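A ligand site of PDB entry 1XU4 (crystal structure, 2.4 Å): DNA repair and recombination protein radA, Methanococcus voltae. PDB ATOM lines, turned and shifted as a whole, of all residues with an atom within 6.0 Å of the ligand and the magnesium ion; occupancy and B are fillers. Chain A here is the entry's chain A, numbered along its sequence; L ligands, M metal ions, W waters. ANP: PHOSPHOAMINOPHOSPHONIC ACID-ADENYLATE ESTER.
Within 4 Å of the magnesium ion: Thr 112.
The side-chain amino group of Lys 318 is in salt-bridge range of the side-chain carboxylate of Glu 317, at 3.9 Å. NH2 of Arg 158 sits at hydrogen-bond distance from O of Glu 317 (2.9 Å). The side-chain amide nitrogen of Gln 257 lies within hydrogen-bond range of the side-chain carboxylate of Glu 151 (3.4 Å). The guanidinium group of Arg 158 lies within hydrogen-bond range of the side-chain amide oxygen of Gln 113 (2.7 Å). O of Gly 108 sits at hydrogen-bond distance from NH2 of Arg 296. The backbone carbonyl oxygen (O) of Thr 316 sits at hydrogen-bond distance from the guanidinium group (NH1) of Arg 158, 2.6 Å away. The backbone NH of Lys 318 sits close to the side-chain hydroxyl of Thr 316. The backbone carbonyl oxygen (O) of Gly 105 sits at hydrogen-bond distance from the side-chain amino group (NZ) of Lys 111, at 3.1 Å.
N of Gly 108 lies close to N3B of the ligand, at 2.8 Å. NH2 of Arg 158 sits close to N6 of the ligand (3.0 Å). Val 106 touches the ligand (O to O2B, 3.999 Å). CA of Phe 107 touches O3G of the ligand, at 3.2 Å. Glu 151 touches the ligand (OE1 to O1G, 3.7 Å). Ile 315 touches the ligand. Thr 316 touches the ligand (C to C2, 3.6 Å). CA of Glu 317 touches N1 of the ligand, at 3.6 Å.
Water W4 lies within hydrogen-bond range of OE1 of Glu 151 (2.6 Å) and OG1 of Thr 153 (2.8 Å). Water W7 bridges OD1 of Asp 211 (2.5 Å) and OG1 of Thr 255 (3.4 Å). Water W6 bridges OE1 of Glu 151 and NE2 of Gln 257. Water W5 lies within hydrogen-bond range of NE2 of Gln 161 (2.7 Å) and N6 of the ligand (3.2 Å). Water W2 lies within hydrogen-bond range of the backbone carbonyl oxygen (O) of Gly 108 (3.0 Å), the guanidinium group (NH2) of Arg 296 (3.0 Å), the backbone NH (N) of Gly 110 (3.2 Å) and an oxygen (O5') of the ligand (3.2 Å).
The magnesium ion is bound by water W4 (2.0 Å), an oxygen (O1G) of the ligand (2.0 Å), water W3 (2.0 Å), an oxygen (O1B) of the ligand (2.2 Å), the side-chain hydroxyl of Thr 112 (2.3 Å) and water W7 (2.5 Å).
NZ of Lys 111 lies within salt-bridge range of O2B of the ligand. O1A of the ligand is in hydrogen-bond range of N of Thr 112 (3.0 Å). The side-chain amide nitrogen of Gln 113 lies close to an oxygen (O1A) of the ligand (3.2 Å). The backbone NH (N) of Gln 113 lies within hydrogen-bond range of an oxygen (O1A) of the ligand (2.8 Å). The backbone NH (N) of Ser 109 lies within hydrogen-bond range of an oxygen (O2B) of the ligand (3.4 Å). The side-chain amide oxygen (OE1) of Gln 161 sits at hydrogen-bond distance from a nitrogen (N6) of the ligand (3.0 Å). The backbone NH (N) of Gly 110 is in hydrogen-bond range of an oxygen (O3A) of the ligand. The backbone NH (N) of Lys 111 is in hydrogen-bond range of an oxygen (O2B) of the ligand.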
ATOM      1  N   GLY A 105      17.243  27.500  15.830  1.00  0.00           N
ATOM      2  CA  GLY A 105      16.271  27.761  16.869  1.00  0.00           C
ATOM      3  C   GLY A 105      16.869  28.031  18.226  1.00  0.00           C
ATOM      4  O   GLY A 105      18.060  27.821  18.476  1.00  0.00           O
ATOM      5  N   VAL A 106      16.008  28.519  19.112  1.00  0.00           N
ATOM      6  CA  VAL A 106      16.372  28.823  20.488  1.00  0.00           C
ATOM      7  C   VAL A 106      16.785  27.527  21.186  1.00  0.00           C
ATOM      8  O   VAL A 106      16.338  26.433  20.810  1.00  0.00           O
ATOM      9  CB  VAL A 106      15.169  29.477  21.228  1.00  0.00           C
ATOM     10  CG1 VAL A 106      13.980  28.512  21.246  1.00  0.00           C
ATOM     11  CG2 VAL A 106      15.551  29.841  22.643  1.00  0.00           C
ATOM     12  N   PHE A 107      17.641  27.652  22.190  1.00  0.00           N
ATOM     13  CA  PHE A 107      18.119  26.509  22.965  1.00  0.00           C
ATOM     14  C   PHE A 107      16.931  25.636  23.365  1.00  0.00           C
ATOM     15  O   PHE A 107      15.842  26.143  23.627  1.00  0.00           O
ATOM     16  CB  PHE A 107      18.829  26.987  24.222  1.00  0.00           C
ATOM     17  CG  PHE A 107      17.890  27.471  25.306  1.00  0.00           C
ATOM     18  CD1 PHE A 107      17.345  26.575  26.241  1.00  0.00           C
ATOM     19  CD2 PHE A 107      17.490  28.808  25.346  1.00  0.00           C
ATOM     20  CE1 PHE A 107      16.415  26.994  27.189  1.00  0.00           C
ATOM     21  CE2 PHE A 107      16.553  29.256  26.301  1.00  0.00           C
ATOM     22  CZ  PHE A 107      16.022  28.345  27.221  1.00  0.00           C
ATOM     23  N   GLY A 108      17.154  24.323  23.409  1.00  0.00           N
ATOM     24  CA  GLY A 108      16.112  23.401  23.806  1.00  0.00           C
ATOM     25  C   GLY A 108      14.924  23.283  22.871  1.00  0.00           C
ATOM     26  O   GLY A 108      13.895  22.736  23.262  1.00  0.00           O
ATOM     27  N   SER A 109      15.039  23.783  21.648  1.00  0.00           N
ATOM     28  CA  SER A 109      13.925  23.688  20.724  1.00  0.00           C
ATOM     29  C   SER A 109      13.827  22.300  20.094  1.00  0.00           C
ATOM     30  O   SER A 109      12.826  21.961  19.478  1.00  0.00           O
ATOM     31  CB  SER A 109      13.995  24.769  19.633  1.00  0.00           C
ATOM     32  OG  SER A 109      15.282  24.862  19.050  1.00  0.00           O
ATOM     33  N   GLY A 110      14.875  21.491  20.288  1.00  0.00           N
ATOM     34  CA  GLY A 110      14.870  20.132  19.777  1.00  0.00           C
ATOM     35  C   GLY A 110      15.678  19.886  18.515  1.00  0.00           C
ATOM     36  O   GLY A 110      15.415  18.930  17.788  1.00  0.00           O
ATOM     37  N   LYS A 111      16.661  20.744  18.255  1.00  0.00           N
ATOM     38  CA  LYS A 111      17.495  20.601  17.065  1.00  0.00           C
ATOM     39  C   LYS A 111      18.286  19.310  17.164  1.00  0.00           C
ATOM     40  O   LYS A 111      18.388  18.550  16.188  1.00  0.00           O
ATOM     41  CB  LYS A 111      18.463  21.786  16.963  1.00  0.00           C
ATOM     42  CG  LYS A 111      17.802  23.154  16.946  1.00  0.00           C
ATOM     43  CD  LYS A 111      18.833  24.270  16.743  1.00  0.00           C
ATOM     44  CE  LYS A 111      19.762  24.436  17.941  1.00  0.00           C
ATOM     45  NZ  LYS A 111      19.011  24.975  19.118  1.00  0.00           N
ATOM     46  N   THR A 112      18.841  19.067  18.334  1.00  0.00           N
ATOM     47  CA  THR A 112      19.634  17.869  18.577  1.00  0.00           C
ATOM     48  C   THR A 112      18.744  16.627  18.538  1.00  0.00           C
ATOM     49  O   THR A 112      19.147  15.590  18.021  1.00  0.00           O
ATOM     50  CB  THR A 112      20.381  17.991  19.910  1.00  0.00           C
ATOM     51  OG1 THR A 112      21.409  18.983  19.763  1.00  0.00           O
ATOM     52  CG2 THR A 112      21.014  16.673  20.324  1.00  0.00           C
ATOM     53  N   GLN A 113      17.535  16.752  19.071  1.00  0.00           N
ATOM     54  CA  GLN A 113      16.581  15.640  19.076  1.00  0.00           C
ATOM     55  C   GLN A 113      16.284  15.204  17.632  1.00  0.00           C
ATOM     56  O   GLN A 113      16.173  14.012  17.340  1.00  0.00           O
ATOM     57  CB  GLN A 113      15.261  16.040  19.740  1.00  0.00           C
ATOM     58  CG  GLN A 113      15.367  16.537  21.174  1.00  0.00           C
ATOM     59  CD  GLN A 113      16.080  15.558  22.079  1.00  0.00           C
ATOM     60  OE1 GLN A 113      15.611  14.432  22.282  1.00  0.00           O
ATOM     61  NE2 GLN A 113      17.215  15.966  22.623  1.00  0.00           N
ATOM     62  N   ILE A 114      16.167  16.181  16.742  1.00  0.00           N
ATOM     63  CA  ILE A 114      15.869  15.911  15.342  1.00  0.00           C
ATOM     64  C   ILE A 114      17.002  15.155  14.678  1.00  0.00           C
ATOM     65  O   ILE A 114      16.761  14.226  13.903  1.00  0.00           O
ATOM     66  CB  ILE A 114      15.585  17.226  14.569  1.00  0.00           C
ATOM     67  CG1 ILE A 114      14.248  17.807  15.036  1.00  0.00           C
ATOM     68  CG2 ILE A 114      15.558  16.967  13.072  1.00  0.00           C
ATOM     69  CD1 ILE A 114      13.936  19.177  14.487  1.00  0.00           C
ATOM     70  N   GLU A 151      29.422  20.095  19.677  1.00  0.00           N
ATOM     71  CA  GLU A 151      29.280  20.628  21.027  1.00  0.00           C
ATOM     72  C   GLU A 151      29.376  19.555  22.130  1.00  0.00           C
ATOM     73  O   GLU A 151      29.363  19.868  23.324  1.00  0.00           O
ATOM     74  CB  GLU A 151      27.952  21.374  21.149  1.00  0.00           C
ATOM     75  CG  GLU A 151      27.302  21.713  19.813  1.00  0.00           C
ATOM     76  CD  GLU A 151      26.292  22.856  19.888  1.00  0.00           C
ATOM     77  OE1 GLU A 151      25.389  22.817  20.749  1.00  0.00           O
ATOM     78  OE2 GLU A 151      26.411  23.804  19.085  1.00  0.00           O
ATOM     79  N   THR A 153      27.152  16.993  22.504  1.00  0.00           N
ATOM     80  CA  THR A 153      25.833  16.612  22.992  1.00  0.00           C
ATOM     81  C   THR A 153      25.234  15.354  22.359  1.00  0.00           C
ATOM     82  O   THR A 153      24.011  15.143  22.433  1.00  0.00           O
ATOM     83  CB  THR A 153      24.808  17.758  22.869  1.00  0.00           C
ATOM     84  OG1 THR A 153      24.895  18.339  21.565  1.00  0.00           O
ATOM     85  CG2 THR A 153      25.057  18.818  23.951  1.00  0.00           C
ATOM     86  N   ARG A 158      19.842   8.319  24.181  1.00  0.00           N
ATOM     87  CA  ARG A 158      18.718   8.871  23.443  1.00  0.00           C
ATOM     88  C   ARG A 158      18.457   8.062  22.153  1.00  0.00           C
ATOM     89  O   ARG A 158      17.301   7.820  21.796  1.00  0.00           O
ATOM     90  CB  ARG A 158      18.995  10.344  23.137  1.00  0.00           C
ATOM     91  CG  ARG A 158      17.785  11.146  22.709  1.00  0.00           C
ATOM     92  CD  ARG A 158      16.672  11.101  23.746  1.00  0.00           C
ATOM     93  NE  ARG A 158      15.523  11.888  23.293  1.00  0.00           N
ATOM     94  CZ  ARG A 158      14.257  11.616  23.571  1.00  0.00           C
ATOM     95  NH1 ARG A 158      13.301  12.397  23.100  1.00  0.00           N
ATOM     96  NH2 ARG A 158      13.938  10.555  24.299  1.00  0.00           N
ATOM     97  N   GLN A 161      16.829   4.859  23.276  1.00  0.00           N
ATOM     98  CA  GLN A 161      15.465   5.168  23.706  1.00  0.00           C
ATOM     99  C   GLN A 161      14.541   5.414  22.519  1.00  0.00           C
ATOM    100  O   GLN A 161      13.476   4.804  22.404  1.00  0.00           O
ATOM    101  CB  GLN A 161      15.532   6.393  24.608  1.00  0.00           C
ATOM    102  CG  GLN A 161      14.254   6.822  25.266  1.00  0.00           C
ATOM    103  CD  GLN A 161      14.516   7.934  26.264  1.00  0.00           C
ATOM    104  OE1 GLN A 161      15.280   8.853  25.983  1.00  0.00           O
ATOM    105  NE2 GLN A 161      13.897   7.844  27.427  1.00  0.00           N
ATOM    106  N   ASP A 211      26.019  19.004  13.851  1.00  0.00           N
ATOM    107  CA  ASP A 211      25.373  19.635  14.998  1.00  0.00           C
ATOM    108  C   ASP A 211      26.436  19.978  16.051  1.00  0.00           C
ATOM    109  O   ASP A 211      26.959  19.068  16.695  1.00  0.00           O
ATOM    110  CB  ASP A 211      24.344  18.659  15.567  1.00  0.00           C
ATOM    111  CG  ASP A 211      23.720  19.128  16.872  1.00  0.00           C
ATOM    112  OD1 ASP A 211      23.524  20.354  17.042  1.00  0.00           O
ATOM    113  OD2 ASP A 211      23.410  18.265  17.718  1.00  0.00           O
ATOM    114  N   THR A 255      22.237  21.944  12.254  1.00  0.00           N
ATOM    115  CA  THR A 255      21.539  22.716  13.268  1.00  0.00           C
ATOM    116  C   THR A 255      22.310  24.043  13.332  1.00  0.00           C
ATOM    117  O   THR A 255      23.486  24.105  12.986  1.00  0.00           O
ATOM    118  CB  THR A 255      21.575  22.019  14.645  1.00  0.00           C
ATOM    119  OG1 THR A 255      22.923  21.928  15.105  1.00  0.00           O
ATOM    120  CG2 THR A 255      20.998  20.619  14.514  1.00  0.00           C
ATOM    121  N   GLN A 257      22.393  28.109  15.534  1.00  0.00           N
ATOM    122  CA  GLN A 257      21.954  28.869  16.694  1.00  0.00           C
ATOM    123  C   GLN A 257      21.348  30.192  16.237  1.00  0.00           C
ATOM    124  O   GLN A 257      21.387  30.524  15.048  1.00  0.00           O
ATOM    125  CB  GLN A 257      23.146  29.093  17.627  1.00  0.00           C
ATOM    126  CG  GLN A 257      23.953  27.824  17.858  1.00  0.00           C
ATOM    127  CD  GLN A 257      24.960  27.950  18.980  1.00  0.00           C
ATOM    128  OE1 GLN A 257      25.644  28.977  19.129  1.00  0.00           O
ATOM    129  NE2 GLN A 257      25.073  26.898  19.791  1.00  0.00           N
ATOM    130  N   VAL A 288      12.806  26.676  14.530  1.00  0.00           N
ATOM    131  CA  VAL A 288      12.038  25.893  15.477  1.00  0.00           C
ATOM    132  C   VAL A 288      11.766  26.682  16.755  1.00  0.00           C
ATOM    133  O   VAL A 288      12.679  27.261  17.350  1.00  0.00           O
ATOM    134  CB  VAL A 288      12.774  24.601  15.834  1.00  0.00           C
ATOM    135  CG1 VAL A 288      12.999  23.783  14.569  1.00  0.00           C
ATOM    136  CG2 VAL A 288      14.106  24.930  16.459  1.00  0.00           C
ATOM    137  N   ARG A 296       6.239  21.895  19.959  1.00  0.00           N
ATOM    138  CA  ARG A 296       7.245  22.620  19.195  1.00  0.00           C
ATOM    139  C   ARG A 296       6.665  23.051  17.848  1.00  0.00           C
ATOM    140  O   ARG A 296       5.732  22.435  17.344  1.00  0.00           O
ATOM    141  CB  ARG A 296       8.478  21.746  18.942  1.00  0.00           C
ATOM    142  CG  ARG A 296       9.219  21.268  20.193  1.00  0.00           C
ATOM    143  CD  ARG A 296      10.016  22.393  20.833  1.00  0.00           C
ATOM    144  NE  ARG A 296      10.785  21.917  21.975  1.00  0.00           N
ATOM    145  CZ  ARG A 296      10.278  21.702  23.189  1.00  0.00           C
ATOM    146  NH1 ARG A 296       8.986  21.931  23.433  1.00  0.00           N
ATOM    147  NH2 ARG A 296      11.065  21.237  24.147  1.00  0.00           N
ATOM    148  N   ILE A 315       8.199  16.728  21.510  1.00  0.00           N
ATOM    149  CA  ILE A 315       9.423  16.006  21.852  1.00  0.00           C
ATOM    150  C   ILE A 315       9.108  15.245  23.139  1.00  0.00           C
ATOM    151  O   ILE A 315       8.977  15.840  24.203  1.00  0.00           O
ATOM    152  CB  ILE A 315      10.630  16.938  22.128  1.00  0.00           C
ATOM    153  CG1 ILE A 315      10.759  18.006  21.036  1.00  0.00           C
ATOM    154  CG2 ILE A 315      11.902  16.098  22.239  1.00  0.00           C
ATOM    155  CD1 ILE A 315      10.906  17.456  19.638  1.00  0.00           C
ATOM    156  N   THR A 316       8.958  13.935  23.030  1.00  0.00           N
ATOM    157  CA  THR A 316       8.638  13.111  24.197  1.00  0.00           C
ATOM    158  C   THR A 316       9.730  12.082  24.386  1.00  0.00           C
ATOM    159  O   THR A 316      10.802  12.208  23.801  1.00  0.00           O
ATOM    160  CB  THR A 316       7.311  12.387  23.992  1.00  0.00           C
ATOM    161  OG1 THR A 316       7.462  11.404  22.962  1.00  0.00           O
ATOM    162  CG2 THR A 316       6.230  13.375  23.575  1.00  0.00           C
ATOM    163  N   GLU A 317       9.478  11.048  25.197  1.00  0.00           N
ATOM    164  CA  GLU A 317      10.493  10.020  25.412  1.00  0.00           C
ATOM    165  C   GLU A 317      10.713   9.230  24.129  1.00  0.00           C
ATOM    166  O   GLU A 317      11.757   8.626  23.925  1.00  0.00           O
ATOM    167  CB  GLU A 317      10.091   9.080  26.552  1.00  0.00           C
ATOM    168  CG  GLU A 317       8.739   9.388  27.205  1.00  0.00           C
ATOM    169  CD  GLU A 317       7.559   8.833  26.430  1.00  0.00           C
ATOM    170  OE1 GLU A 317       7.482   7.598  26.263  1.00  0.00           O
ATOM    171  OE2 GLU A 317       6.705   9.637  25.981  1.00  0.00           O
ATOM    172  N   LYS A 318       9.714   9.266  23.258  1.00  0.00           N
ATOM    173  CA  LYS A 318       9.770   8.566  21.974  1.00  0.00           C
ATOM    174  C   LYS A 318      10.623   9.296  20.944  1.00  0.00           C
ATOM    175  O   LYS A 318      11.061   8.714  19.947  1.00  0.00           O
ATOM    176  CB  LYS A 318       8.362   8.402  21.394  1.00  0.00           C
ATOM    177  CG  LYS A 318       7.608   7.191  21.909  1.00  0.00           C
ATOM    178  CD  LYS A 318       6.442   7.604  22.785  1.00  0.00           C
ATOM    179  CE  LYS A 318       5.614   6.400  23.169  1.00  0.00           C
ATOM    180  NZ  LYS A 318       4.417   6.800  23.940  1.00  0.00           N
HETATM  181  PG  ANP L   1      20.753  23.735  22.071  1.00  0.00           P
HETATM  182  O1G ANP L   1      21.703  22.966  21.329  1.00  0.00           O
HETATM  183  O2G ANP L   1      21.343  24.060  23.391  1.00  0.00           O
HETATM  184  O3G ANP L   1      20.480  24.970  21.378  1.00  0.00           O
HETATM  185  PB  ANP L   1      18.598  21.975  21.182  1.00  0.00           P
HETATM  186  O1B ANP L   1      19.570  21.048  20.519  1.00  0.00           O
HETATM  187  O2B ANP L   1      17.971  22.836  20.185  1.00  0.00           O
HETATM  188  N3B ANP L   1      19.316  22.871  22.294  1.00  0.00           N
HETATM  189  PA  ANP L   1      17.582  19.579  22.334  1.00  0.00           P
HETATM  190  O1A ANP L   1      17.639  18.690  21.073  1.00  0.00           O
HETATM  191  O2A ANP L   1      18.806  19.385  23.129  1.00  0.00           O
HETATM  192  O3A ANP L   1      17.419  21.133  21.893  1.00  0.00           O
HETATM  193  O5' ANP L   1      16.248  19.163  23.209  1.00  0.00           O
HETATM  194  C5' ANP L   1      16.165  19.435  24.702  1.00  0.00           C
HETATM  195  C4' ANP L   1      14.955  19.079  25.126  1.00  0.00           C
HETATM  196  O4' ANP L   1      14.611  17.718  24.639  1.00  0.00           O
HETATM  197  C3' ANP L   1      14.956  18.873  26.661  1.00  0.00           C
HETATM  198  O3' ANP L   1      15.202  20.000  27.419  1.00  0.00           O
HETATM  199  C2' ANP L   1      13.792  17.870  26.903  1.00  0.00           C
HETATM  200  O2' ANP L   1      12.489  18.657  27.112  1.00  0.00           O
HETATM  201  C1' ANP L   1      13.680  17.117  25.568  1.00  0.00           C
HETATM  202  N9  ANP L   1      14.088  15.867  25.836  1.00  0.00           N
HETATM  203  C8  ANP L   1      15.395  15.348  25.724  1.00  0.00           C
HETATM  204  N7  ANP L   1      15.404  14.122  26.095  1.00  0.00           N
HETATM  205  C5  ANP L   1      14.159  13.764  26.474  1.00  0.00           C
HETATM  206  C6  ANP L   1      13.604  12.589  26.962  1.00  0.00           C
HETATM  207  N6  ANP L   1      14.372  11.494  27.151  1.00  0.00           N
HETATM  208  N1  ANP L   1      12.211  12.558  27.264  1.00  0.00           N
HETATM  209  C2  ANP L   1      11.384  13.709  27.074  1.00  0.00           C
HETATM  210  N3  ANP L   1      11.914  14.878  26.604  1.00  0.00           N
HETATM  211  C4  ANP L   1      13.318  14.853  26.315  1.00  0.00           C
HETATM  212 MG    MG M   1      21.784  21.033  20.668  1.00  0.00          MG
HETATM  213  O   HOH W   1      12.611  21.016  27.889  1.00  0.00           O
HETATM  214  O   HOH W   2      13.206  19.904  22.478  1.00  0.00           O
HETATM  215  O   HOH W   3      21.508  20.087  22.462  1.00  0.00           O
HETATM  216  O   HOH W   4      23.748  20.788  20.677  1.00  0.00           O
HETATM  217  O   HOH W   5      13.586   9.491  29.506  1.00  0.00           O
HETATM  218  O   HOH W   6      23.225  24.243  19.317  1.00  0.00           O
HETATM  219  O   HOH W   7      21.967  21.770  18.313  1.00  0.00           O
